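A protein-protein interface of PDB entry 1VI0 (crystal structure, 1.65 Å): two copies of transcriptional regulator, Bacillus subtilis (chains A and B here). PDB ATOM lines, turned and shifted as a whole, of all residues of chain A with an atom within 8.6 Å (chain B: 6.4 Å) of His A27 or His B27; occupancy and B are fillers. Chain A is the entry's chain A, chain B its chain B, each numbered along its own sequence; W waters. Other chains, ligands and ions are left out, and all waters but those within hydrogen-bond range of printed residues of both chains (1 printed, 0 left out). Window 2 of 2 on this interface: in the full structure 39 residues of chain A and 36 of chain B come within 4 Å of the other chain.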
ATOM      1  N   VAL A  20     -10.158  -8.072   8.633  1.00  0.00           N
ATOM      2  CA  VAL A  20     -10.932  -9.284   8.435  1.00  0.00           C
ATOM      3  C   VAL A  20     -10.051 -10.495   8.231  1.00  0.00           C
ATOM      4  O   VAL A  20     -10.261 -11.535   8.857  1.00  0.00           O
ATOM      5  CB  VAL A  20     -11.908  -9.115   7.245  1.00  0.00           C
ATOM      6  CG1 VAL A  20     -12.589 -10.422   6.932  1.00  0.00           C
ATOM      7  CG2 VAL A  20     -12.904  -7.995   7.507  1.00  0.00           C
ATOM      8  N   ILE A  21      -9.026 -10.347   7.396  1.00  0.00           N
ATOM      9  CA  ILE A  21      -8.088 -11.457   7.112  1.00  0.00           C
ATOM     10  C   ILE A  21      -7.321 -11.833   8.379  1.00  0.00           C
ATOM     11  O   ILE A  21      -7.137 -13.024   8.690  1.00  0.00           O
ATOM     12  CB  ILE A  21      -7.148 -11.077   5.981  1.00  0.00           C
ATOM     13  CG1 ILE A  21      -7.850 -10.985   4.609  1.00  0.00           C
ATOM     14  CG2 ILE A  21      -5.947 -11.979   5.888  1.00  0.00           C
ATOM     15  CD1 ILE A  21      -7.100 -10.060   3.664  1.00  0.00           C
ATOM     16  N   ASN A  24     -10.185 -13.435  10.731  1.00  0.00           N
ATOM     17  CA  ASN A  24     -10.814 -14.675  10.279  1.00  0.00           C
ATOM     18  C   ASN A  24      -9.951 -15.678   9.571  1.00  0.00           C
ATOM     19  O   ASN A  24     -10.367 -16.864   9.482  1.00  0.00           O
ATOM     20  CB  ASN A  24     -11.984 -14.269   9.317  1.00  0.00           C
ATOM     21  CG  ASN A  24     -13.081 -13.558  10.116  1.00  0.00           C
ATOM     22  OD1 ASN A  24     -13.949 -14.239  10.654  1.00  0.00           O
ATOM     23  ND2 ASN A  24     -13.013 -12.251  10.258  1.00  0.00           N
ATOM     24  N   GLY A  25      -8.763 -15.345   9.107  1.00  0.00           N
ATOM     25  CA  GLY A  25      -7.924 -16.245   8.296  1.00  0.00           C
ATOM     26  C   GLY A  25      -8.326 -15.921   6.821  1.00  0.00           C
ATOM     27  O   GLY A  25      -9.497 -15.603   6.595  1.00  0.00           O
ATOM     28  N   TYR A  26      -7.376 -15.886   5.915  1.00  0.00           N
ATOM     29  CA  TYR A  26      -7.597 -15.531   4.541  1.00  0.00           C
ATOM     30  C   TYR A  26      -8.689 -16.386   3.888  1.00  0.00           C
ATOM     31  O   TYR A  26      -9.502 -15.870   3.149  1.00  0.00           O
ATOM     32  CB  TYR A  26      -6.308 -15.720   3.732  1.00  0.00           C
ATOM     33  CG  TYR A  26      -6.504 -15.541   2.241  1.00  0.00           C
ATOM     34  CD1 TYR A  26      -6.898 -14.329   1.667  1.00  0.00           C
ATOM     35  CD2 TYR A  26      -6.295 -16.628   1.407  1.00  0.00           C
ATOM     36  CE1 TYR A  26      -7.052 -14.215   0.299  1.00  0.00           C
ATOM     37  CE2 TYR A  26      -6.415 -16.522   0.038  1.00  0.00           C
ATOM     38  CZ  TYR A  26      -6.789 -15.319  -0.509  1.00  0.00           C
ATOM     39  OH  TYR A  26      -6.926 -15.239  -1.875  1.00  0.00           O
ATOM     40  N   HIS A  27      -8.678 -17.690   4.151  1.00  0.00           N
ATOM     41  CA  HIS A  27      -9.675 -18.568   3.502  1.00  0.00           C
ATOM     42  C   HIS A  27     -11.082 -18.250   3.897  1.00  0.00           C
ATOM     43  O   HIS A  27     -12.026 -18.470   3.096  1.00  0.00           O
ATOM     44  CB  HIS A  27      -9.280 -20.033   3.758  1.00  0.00           C
ATOM     45  CG  HIS A  27      -8.050 -20.339   2.915  1.00  0.00           C
ATOM     46  ND1 HIS A  27      -8.091 -20.199   1.537  1.00  0.00           N
ATOM     47  CD2 HIS A  27      -6.809 -20.709   3.228  1.00  0.00           C
ATOM     48  CE1 HIS A  27      -6.905 -20.498   1.038  1.00  0.00           C
ATOM     49  NE2 HIS A  27      -6.103 -20.813   2.046  1.00  0.00           N
ATOM     50  N   GLN A  28     -11.304 -17.675   5.065  1.00  0.00           N
ATOM     51  CA  GLN A  28     -12.629 -17.293   5.539  1.00  0.00           C
ATOM     52  C   GLN A  28     -12.926 -15.819   5.390  1.00  0.00           C
ATOM     53  O   GLN A  28     -13.893 -15.309   5.963  1.00  0.00           O
ATOM     54  CB  GLN A  28     -12.746 -17.698   7.025  1.00  0.00           C
ATOM     55  CG  GLN A  28     -12.229 -19.116   7.278  1.00  0.00           C
ATOM     56  N   SER A  29     -12.135 -15.071   4.651  1.00  0.00           N
ATOM     57  CA  SER A  29     -12.276 -13.674   4.387  1.00  0.00           C
ATOM     58  C   SER A  29     -12.878 -13.357   3.018  1.00  0.00           C
ATOM     59  O   SER A  29     -12.252 -12.731   2.142  1.00  0.00           O
ATOM     60  CB  SER A  29     -10.878 -12.995   4.478  1.00  0.00           C
ATOM     61  OG  SER A  29     -10.326 -13.234   5.758  1.00  0.00           O
ATOM     62  N   GLN A  30     -14.168 -13.649   2.831  1.00  0.00           N
ATOM     63  CA  GLN A  30     -14.806 -13.359   1.563  1.00  0.00           C
ATOM     64  C   GLN A  30     -15.121 -11.885   1.375  1.00  0.00           C
ATOM     65  O   GLN A  30     -15.305 -11.117   2.306  1.00  0.00           O
ATOM     66  CB  GLN A  30     -16.087 -14.205   1.372  1.00  0.00           C
ATOM     67  CG  GLN A  30     -16.539 -14.222  -0.098  1.00  0.00           C
ATOM     68  CD  GLN A  30     -15.404 -14.616  -1.028  1.00  0.00           C
ATOM     69  OE1 GLN A  30     -15.109 -13.946  -2.025  1.00  0.00           O
ATOM     70  NE2 GLN A  30     -14.742 -15.725  -0.677  1.00  0.00           N
ATOM     71  N   VAL A  31     -15.245 -11.487   0.109  1.00  0.00           N
ATOM     72  CA  VAL A  31     -15.576 -10.130  -0.274  1.00  0.00           C
ATOM     73  C   VAL A  31     -16.725  -9.549   0.511  1.00  0.00           C
ATOM     74  O   VAL A  31     -16.634  -8.435   1.077  1.00  0.00           O
ATOM     75  CB  VAL A  31     -15.828 -10.091  -1.801  1.00  0.00           C
ATOM     76  CG1 VAL A  31     -16.223  -8.709  -2.289  1.00  0.00           C
ATOM     77  CG2 VAL A  31     -14.550 -10.540  -2.523  1.00  0.00           C
ATOM     78  N   LYS A  33     -17.712 -10.172   3.548  1.00  0.00           N
ATOM     79  CA  LYS A  33     -17.287  -9.864   4.919  1.00  0.00           C
ATOM     80  C   LYS A  33     -16.440  -8.597   4.952  1.00  0.00           C
ATOM     81  O   LYS A  33     -16.580  -7.752   5.841  1.00  0.00           O
ATOM     82  CB  LYS A  33     -16.517 -11.060   5.505  1.00  0.00           C
ATOM     83  CG  LYS A  33     -17.276 -12.380   5.420  1.00  0.00           C
ATOM     84  CD  LYS A  33     -16.581 -13.494   6.185  1.00  0.00           C
ATOM     85  CE  LYS A  33     -17.182 -14.850   5.813  1.00  0.00           C
ATOM     86  NZ  LYS A  33     -18.678 -14.792   5.869  1.00  0.00           N
ATOM     87  N   LYS A  52     -10.942 -11.797  -4.148  1.00  0.00           N
ATOM     88  CA  LYS A  52     -10.286 -11.891  -2.817  1.00  0.00           C
ATOM     89  C   LYS A  52      -8.778 -11.946  -2.973  1.00  0.00           C
ATOM     90  O   LYS A  52      -7.984 -11.211  -2.340  1.00  0.00           O
ATOM     91  CB  LYS A  52     -10.758 -13.192  -2.153  1.00  0.00           C
ATOM     92  CG  LYS A  52     -10.507 -13.338  -0.693  1.00  0.00           C
ATOM     93  CD  LYS A  52     -11.221 -14.548  -0.099  1.00  0.00           C
ATOM     94  CE  LYS A  52     -10.482 -15.831  -0.357  1.00  0.00           C
ATOM     95  NZ  LYS A  52     -10.785 -16.860   0.684  1.00  0.00           N
ATOM     96  N   GLU A  53      -8.310 -12.850  -3.816  1.00  0.00           N
ATOM     97  CA  GLU A  53      -6.883 -12.940  -4.116  1.00  0.00           C
ATOM     98  C   GLU A  53      -6.306 -11.599  -4.507  1.00  0.00           C
ATOM     99  O   GLU A  53      -5.238 -11.211  -3.980  1.00  0.00           O
ATOM    100  CB  GLU A  53      -6.654 -14.046  -5.134  1.00  0.00           C
ATOM    101  CG  GLU A  53      -5.229 -14.324  -5.509  1.00  0.00           C
ATOM    102  CD  GLU A  53      -5.146 -15.430  -6.571  1.00  0.00           C
ATOM    103  OE1 GLU A  53      -5.425 -16.593  -6.239  1.00  0.00           O
ATOM    104  OE2 GLU A  53      -4.768 -15.051  -7.695  1.00  0.00           O
ATOM    105  N   LEU A  56      -5.750  -9.441  -1.440  1.00  0.00           N
ATOM    106  CA  LEU A  56      -4.571  -9.884  -0.637  1.00  0.00           C
ATOM    107  C   LEU A  56      -3.275  -9.381  -1.244  1.00  0.00           C
ATOM    108  O   LEU A  56      -2.355  -8.821  -0.623  1.00  0.00           O
ATOM    109  CB  LEU A  56      -4.531 -11.384  -0.556  1.00  0.00           C
ATOM    110  CG  LEU A  56      -3.385 -11.939   0.348  1.00  0.00           C
ATOM    111  CD1 LEU A  56      -3.705 -11.630   1.800  1.00  0.00           C
ATOM    112  CD2 LEU A  56      -3.331 -13.455   0.119  1.00  0.00           C
ATOM    113  N   LEU A 108       1.448 -14.795   8.889  1.00  0.00           N
ATOM    114  CA  LEU A 108       0.604 -15.956   8.728  1.00  0.00           C
ATOM    115  C   LEU A 108      -0.220 -15.926   7.452  1.00  0.00           C
ATOM    116  O   LEU A 108      -0.012 -16.820   6.599  1.00  0.00           O
ATOM    117  CB  LEU A 108      -0.361 -16.090   9.922  1.00  0.00           C
ATOM    118  CG  LEU A 108      -0.030 -17.029  11.062  1.00  0.00           C
ATOM    119  CD1 LEU A 108       1.397 -17.482  11.144  1.00  0.00           C
ATOM    120  CD2 LEU A 108      -0.474 -16.401  12.413  1.00  0.00           C
ATOM    121  N   GLU A 109      -1.083 -14.935   7.281  1.00  0.00           N
ATOM    122  CA  GLU A 109      -2.032 -14.948   6.158  1.00  0.00           C
ATOM    123  C   GLU A 109      -1.493 -14.796   4.776  1.00  0.00           C
ATOM    124  O   GLU A 109      -2.074 -15.313   3.801  1.00  0.00           O
ATOM    125  CB  GLU A 109      -3.183 -13.973   6.463  1.00  0.00           C
ATOM    126  CG  GLU A 109      -3.853 -14.292   7.812  1.00  0.00           C
ATOM    127  CD  GLU A 109      -4.445 -15.672   7.886  1.00  0.00           C
ATOM    128  OE1 GLU A 109      -4.761 -16.302   6.821  1.00  0.00           O
ATOM    129  OE2 GLU A 109      -4.595 -16.183   9.003  1.00  0.00           O
ATOM    130  N   ARG A 111       1.193 -16.154   3.700  1.00  0.00           N
ATOM    131  CA  ARG A 111       2.035 -17.312   3.471  1.00  0.00           C
ATOM    132  C   ARG A 111       1.259 -18.460   2.801  1.00  0.00           C
ATOM    133  O   ARG A 111       1.194 -19.569   3.352  1.00  0.00           O
ATOM    134  CB  ARG A 111       2.634 -17.810   4.797  1.00  0.00           C
ATOM    135  CG  ARG A 111       3.186 -16.704   5.698  1.00  0.00           C
ATOM    136  CD  ARG A 111       4.678 -16.504   5.627  1.00  0.00           C
ATOM    137  NE  ARG A 111       5.091 -15.186   6.110  1.00  0.00           N
ATOM    138  CZ  ARG A 111       6.268 -14.830   6.578  1.00  0.00           C
ATOM    139  NH1 ARG A 111       7.260 -15.712   6.672  1.00  0.00           N
ATOM    140  NH2 ARG A 111       6.493 -13.571   6.943  1.00  0.00           N
ATOM    141  N   GLN A 112       0.595 -18.109   1.717  1.00  0.00           N
ATOM    142  CA  GLN A 112      -0.249 -19.059   0.981  1.00  0.00           C
ATOM    143  C   GLN A 112       0.680 -20.078   0.319  1.00  0.00           C
ATOM    144  O   GLN A 112       1.770 -19.695  -0.120  1.00  0.00           O
ATOM    145  CB  GLN A 112      -1.115 -18.302  -0.011  1.00  0.00           C
ATOM    146  CG  GLN A 112      -2.104 -17.334   0.663  1.00  0.00           C
ATOM    147  CD  GLN A 112      -3.083 -18.070   1.566  1.00  0.00           C
ATOM    148  OE1 GLN A 112      -3.633 -19.120   1.203  1.00  0.00           O
ATOM    149  NE2 GLN A 112      -3.298 -17.561   2.774  1.00  0.00           N
ATOM    150  N   SER A 113       0.288 -21.354   0.346  1.00  0.00           N
ATOM    151  CA  SER A 113       1.120 -22.405  -0.203  1.00  0.00           C
ATOM    152  C   SER A 113       0.718 -22.738  -1.626  1.00  0.00           C
ATOM    153  O   SER A 113       1.476 -23.354  -2.383  1.00  0.00           O
ATOM    154  CB  SER A 113       1.081 -23.662   0.674  1.00  0.00           C
ATOM    155  OG  SER A 113      -0.250 -24.169   0.684  1.00  0.00           O
ATOM    156  N   ASN A 114      -0.490 -22.295  -2.012  1.00  0.00           N
ATOM    157  CA  ASN A 114      -0.774 -22.520  -3.464  1.00  0.00           C
ATOM    158  C   ASN A 114       0.397 -21.822  -4.180  1.00  0.00           C
ATOM    159  O   ASN A 114       0.765 -20.719  -3.746  1.00  0.00           O
ATOM    160  CB  ASN A 114      -2.074 -21.869  -3.865  1.00  0.00           C
ATOM    161  CG  ASN A 114      -2.419 -22.268  -5.303  1.00  0.00           C
ATOM    162  OD1 ASN A 114      -2.235 -21.485  -6.219  1.00  0.00           O
ATOM    163  ND2 ASN A 114      -2.892 -23.505  -5.417  1.00  0.00           N
ATOM    164  N   LEU A 117      -0.390 -18.339  -6.620  1.00  0.00           N
ATOM    165  CA  LEU A 117      -0.584 -17.175  -5.775  1.00  0.00           C
ATOM    166  C   LEU A 117       0.676 -16.768  -5.014  1.00  0.00           C
ATOM    167  O   LEU A 117       1.018 -15.581  -4.947  1.00  0.00           O
ATOM    168  CB  LEU A 117      -1.707 -17.447  -4.776  1.00  0.00           C
ATOM    169  CG  LEU A 117      -2.025 -16.355  -3.763  1.00  0.00           C
ATOM    170  CD1 LEU A 117      -2.231 -15.010  -4.448  1.00  0.00           C
ATOM    171  CD2 LEU A 117      -3.242 -16.721  -2.935  1.00  0.00           C
ATOM    172  N   ASN B  24      -1.228 -29.147  -4.872  1.00  0.00           N
ATOM    173  CA  ASN B  24      -2.236 -28.093  -4.844  1.00  0.00           C
ATOM    174  C   ASN B  24      -2.166 -27.191  -3.614  1.00  0.00           C
ATOM    175  O   ASN B  24      -2.587 -26.022  -3.610  1.00  0.00           O
ATOM    176  CB  ASN B  24      -3.610 -28.778  -4.916  1.00  0.00           C
ATOM    177  CG  ASN B  24      -3.767 -30.019  -5.742  1.00  0.00           C
ATOM    178  OD1 ASN B  24      -3.521 -30.071  -6.964  1.00  0.00           O
ATOM    179  ND2 ASN B  24      -4.264 -31.122  -5.158  1.00  0.00           N
ATOM    180  N   GLY B  25      -1.504 -27.647  -2.566  1.00  0.00           N
ATOM    181  CA  GLY B  25      -1.453 -26.900  -1.298  1.00  0.00           C
ATOM    182  C   GLY B  25      -2.360 -27.673  -0.336  1.00  0.00           C
ATOM    183  O   GLY B  25      -3.299 -28.322  -0.807  1.00  0.00           O
ATOM    184  N   TYR B  26      -2.083 -27.606   0.958  1.00  0.00           N
ATOM    185  CA  TYR B  26      -2.871 -28.314   1.956  1.00  0.00           C
ATOM    186  C   TYR B  26      -4.341 -27.961   1.918  1.00  0.00           C
ATOM    187  O   TYR B  26      -5.200 -28.853   1.967  1.00  0.00           O
ATOM    188  CB  TYR B  26      -2.303 -28.009   3.373  1.00  0.00           C
ATOM    189  CG  TYR B  26      -3.179 -28.583   4.468  1.00  0.00           C
ATOM    190  CD1 TYR B  26      -3.310 -29.957   4.621  1.00  0.00           C
ATOM    191  CD2 TYR B  26      -3.904 -27.748   5.300  1.00  0.00           C
ATOM    192  CE1 TYR B  26      -4.144 -30.482   5.591  1.00  0.00           C
ATOM    193  CE2 TYR B  26      -4.731 -28.263   6.284  1.00  0.00           C
ATOM    194  CZ  TYR B  26      -4.826 -29.621   6.436  1.00  0.00           C
ATOM    195  OH  TYR B  26      -5.651 -30.161   7.411  1.00  0.00           O
ATOM    196  N   HIS B  27      -4.658 -26.664   1.852  1.00  0.00           N
ATOM    197  CA  HIS B  27      -6.004 -26.177   1.855  1.00  0.00           C
ATOM    198  C   HIS B  27      -6.857 -26.835   0.753  1.00  0.00           C
ATOM    199  O   HIS B  27      -7.984 -27.229   1.029  1.00  0.00           O
ATOM    200  CB  HIS B  27      -6.122 -24.668   1.713  1.00  0.00           C
ATOM    201  CG  HIS B  27      -7.517 -24.162   1.987  1.00  0.00           C
ATOM    202  ND1 HIS B  27      -8.288 -23.562   1.033  1.00  0.00           N
ATOM    203  CD2 HIS B  27      -8.247 -24.154   3.132  1.00  0.00           C
ATOM    204  CE1 HIS B  27      -9.452 -23.204   1.553  1.00  0.00           C
ATOM    205  NE2 HIS B  27      -9.455 -23.545   2.828  1.00  0.00           N
ATOM    206  N   GLN B  28      -6.320 -26.869  -0.446  1.00  0.00           N
ATOM    207  CA  GLN B  28      -7.049 -27.475  -1.577  1.00  0.00           C
ATOM    208  C   GLN B  28      -7.011 -28.987  -1.590  1.00  0.00           C
ATOM    209  O   GLN B  28      -7.883 -29.649  -2.205  1.00  0.00           O
ATOM    210  CB  GLN B  28      -6.398 -26.940  -2.868  1.00  0.00           C
ATOM    211  CG  GLN B  28      -6.957 -25.577  -3.284  1.00  0.00           C
ATOM    212  CD  GLN B  28      -5.974 -24.890  -4.234  1.00  0.00           C
ATOM    213  OE1 GLN B  28      -5.709 -25.409  -5.315  1.00  0.00           O
ATOM    214  NE2 GLN B  28      -5.409 -23.777  -3.790  1.00  0.00           N
ATOM    215  N   SER B  29      -5.992 -29.597  -1.007  1.00  0.00           N
ATOM    216  CA  SER B  29      -5.829 -31.038  -1.011  1.00  0.00           C
ATOM    217  C   SER B  29      -7.083 -31.730  -0.495  1.00  0.00           C
ATOM    218  O   SER B  29      -7.810 -31.263   0.380  1.00  0.00           O
ATOM    219  CB  SER B  29      -4.573 -31.482  -0.281  1.00  0.00           C
ATOM    220  OG  SER B  29      -4.712 -31.478   1.131  1.00  0.00           O
ATOM    221  N   GLN B  30      -7.408 -32.854  -1.162  1.00  0.00           N
ATOM    222  CA  GLN B  30      -8.621 -33.597  -0.784  1.00  0.00           C
ATOM    223  C   GLN B  30      -8.238 -34.977  -0.300  1.00  0.00           C
ATOM    224  O   GLN B  30      -7.376 -35.637  -0.918  1.00  0.00           O
ATOM    225  CB  GLN B  30      -9.557 -33.642  -2.002  1.00  0.00           C
ATOM    226  CG  GLN B  30     -10.108 -32.278  -2.411  1.00  0.00           C
ATOM    227  CD  GLN B  30     -11.187 -32.345  -3.461  1.00  0.00           C
ATOM    228  OE1 GLN B  30     -12.275 -31.769  -3.309  1.00  0.00           O
ATOM    229  NE2 GLN B  30     -10.938 -33.045  -4.571  1.00  0.00           N
ATOM    230  N   LYS B  52      -8.139 -34.941   7.763  1.00  0.00           N
ATOM    231  CA  LYS B  52      -7.130 -34.267   6.930  1.00  0.00           C
ATOM    232  C   LYS B  52      -6.012 -33.662   7.758  1.00  0.00           C
ATOM    233  O   LYS B  52      -4.817 -33.825   7.465  1.00  0.00           O
ATOM    234  CB  LYS B  52      -7.855 -33.165   6.182  1.00  0.00           C
ATOM    235  CG  LYS B  52      -7.313 -32.752   4.846  1.00  0.00           C
ATOM    236  CD  LYS B  52      -7.868 -31.375   4.490  1.00  0.00           C
ATOM    237  CE  LYS B  52      -7.290 -30.836   3.206  1.00  0.00           C
ATOM    238  NZ  LYS B  52      -7.926 -29.525   2.830  1.00  0.00           N
ATOM    239  N   GLU B 109       3.846 -25.362   4.404  1.00  0.00           N
ATOM    240  CA  GLU B 109       2.718 -25.708   5.288  1.00  0.00           C
ATOM    241  C   GLU B 109       3.147 -25.623   6.760  1.00  0.00           C
ATOM    242  O   GLU B 109       2.455 -26.119   7.651  1.00  0.00           O
ATOM    243  CB  GLU B 109       2.261 -27.140   4.991  1.00  0.00           C
ATOM    244  CG  GLU B 109       1.788 -27.355   3.560  1.00  0.00           C
ATOM    245  CD  GLU B 109       0.698 -26.462   3.102  1.00  0.00           C
ATOM    246  OE1 GLU B 109      -0.010 -25.825   3.950  1.00  0.00           O
ATOM    247  OE2 GLU B 109       0.407 -26.367   1.881  1.00  0.00           O
ATOM    248  N   SER B 113      -2.607 -20.968   9.499  1.00  0.00           N
ATOM    249  CA  SER B 113      -3.482 -19.929  10.081  1.00  0.00           C
ATOM    250  C   SER B 113      -4.326 -20.472  11.218  1.00  0.00           C
ATOM    251  O   SER B 113      -4.491 -19.833  12.267  1.00  0.00           O
ATOM    252  CB  SER B 113      -4.375 -19.361   8.966  1.00  0.00           C
ATOM    253  OG  SER B 113      -5.432 -18.596   9.572  1.00  0.00           O
HETATM  254  O   HOH W   1      -2.832 -24.784   2.894  1.00  0.00           O
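ND2 of Asn A114 is in hydrogen-bond range of O of Asn B24, 3.1 Å away. OG of Ser B113 is in hydrogen-bond range of OE2 of Glu A109 (2.6 Å). A ring nitrogen (ND1) of His A27 sits close to a ring nitrogen (ND1) of His B27, 3.4 Å away. ND2 of Asn A114 lies close to NE2 of Gln B28 (3.0 Å). OG of Ser A113 is in hydrogen-bond range of OE2 of Glu B109.
The backbone NH of Tyr B26 is in hydrogen-bond range of the side-chain carboxylate of Glu B109 (2.9 Å). NE2 of His A27 lies within hydrogen-bond range of OE1 of Gln A112, at 3.1 Å. O of Tyr B26 lies within hydrogen-bond range of OG of Ser B29 (2.8 Å). The backbone NH (N) of Tyr A26 is in hydrogen-bond range of the side-chain carboxylate (OE1) of Glu A109 (2.8 Å). O of Gly A25 is in hydrogen-bond range of OG of Ser A29, at 2.6 Å. The backbone carbonyl oxygen (O) of His B27 is in hydrogen-bond range of the side-chain amino group (NZ) of Lys B52 (2.9 Å).
Gly A25 touches Ser B113 (CA to OG, 3.7 Å). CA of Gly B25 touches OG of Ser A113, 3.6 Å away. Ser A113 touches Tyr B26 (OG to N, 3.9 Å).
Leu A56 touches none of the printed residues of chain B. Printed residues of chain B within 4 Å of Asn A114: Asn B24 and Gln B28. Of chain A, only His A27 (3.3 Å) comes within 4 Å of His B27. Of the printed residues of chain A, Glu B109 touches Ser A113 (2.6 Å). Of the printed residues of chain A, Ser B113 touches Gly A25 and Glu A109. The nearest residue of chain B that does not touch His A27 is Gln B28 (6.0 Å). The nearest residue of chain A that does not touch His B27 is Ser A113 (5.2 Å). The nearest printed residue of chain A that does not touch Gly B25 is Asn A114 (4.8 Å).
Printed residues of chain B that touch a printed residue of chain A: Asn B24, Gly B25, Tyr B26, His B27, Gln B28, Glu B109 and Ser B113. Hydrophobic or aromatic side chains of chain B within 4 Å of the printed part of chain A: His B27. Of the 21 printed residues of chain A, 5 touch a printed residue of chain B. Hydrophobic or aromatic side chains of chain A within 4 Å of the printed part of chain B: His A27. Along chain A the printed residues that touch a printed residue of chain B span positions 25 to 114.
Gly A25 touches Ser B113, and with the chains exchanged Ser A113 touches Gly B25. His B27 touches its own counterpart, His A27. Glu A109 touches Ser B113, and with the chains exchanged Ser A113 touches Glu B109. Ser A113 touches Tyr B26, but with the chains exchanged Tyr A26 does not touch Ser B113 (4.9 Å). Positions printed for both chains: 24, 25, 26, 27, 28, 29, 30, 52, 109 and 113. Of the 8 pairs that touch across the chains among the printed residues, 5 have their exchanged pair printed and touching as well.
Water W1 lies within hydrogen-bond range of the backbone NH (N) of His B27 (2.8 Å), the side-chain carboxylate (OE1) of Glu B109 (3.2 Å) and the side-chain hydroxyl (OG) of Ser A113 (3.5 Å).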
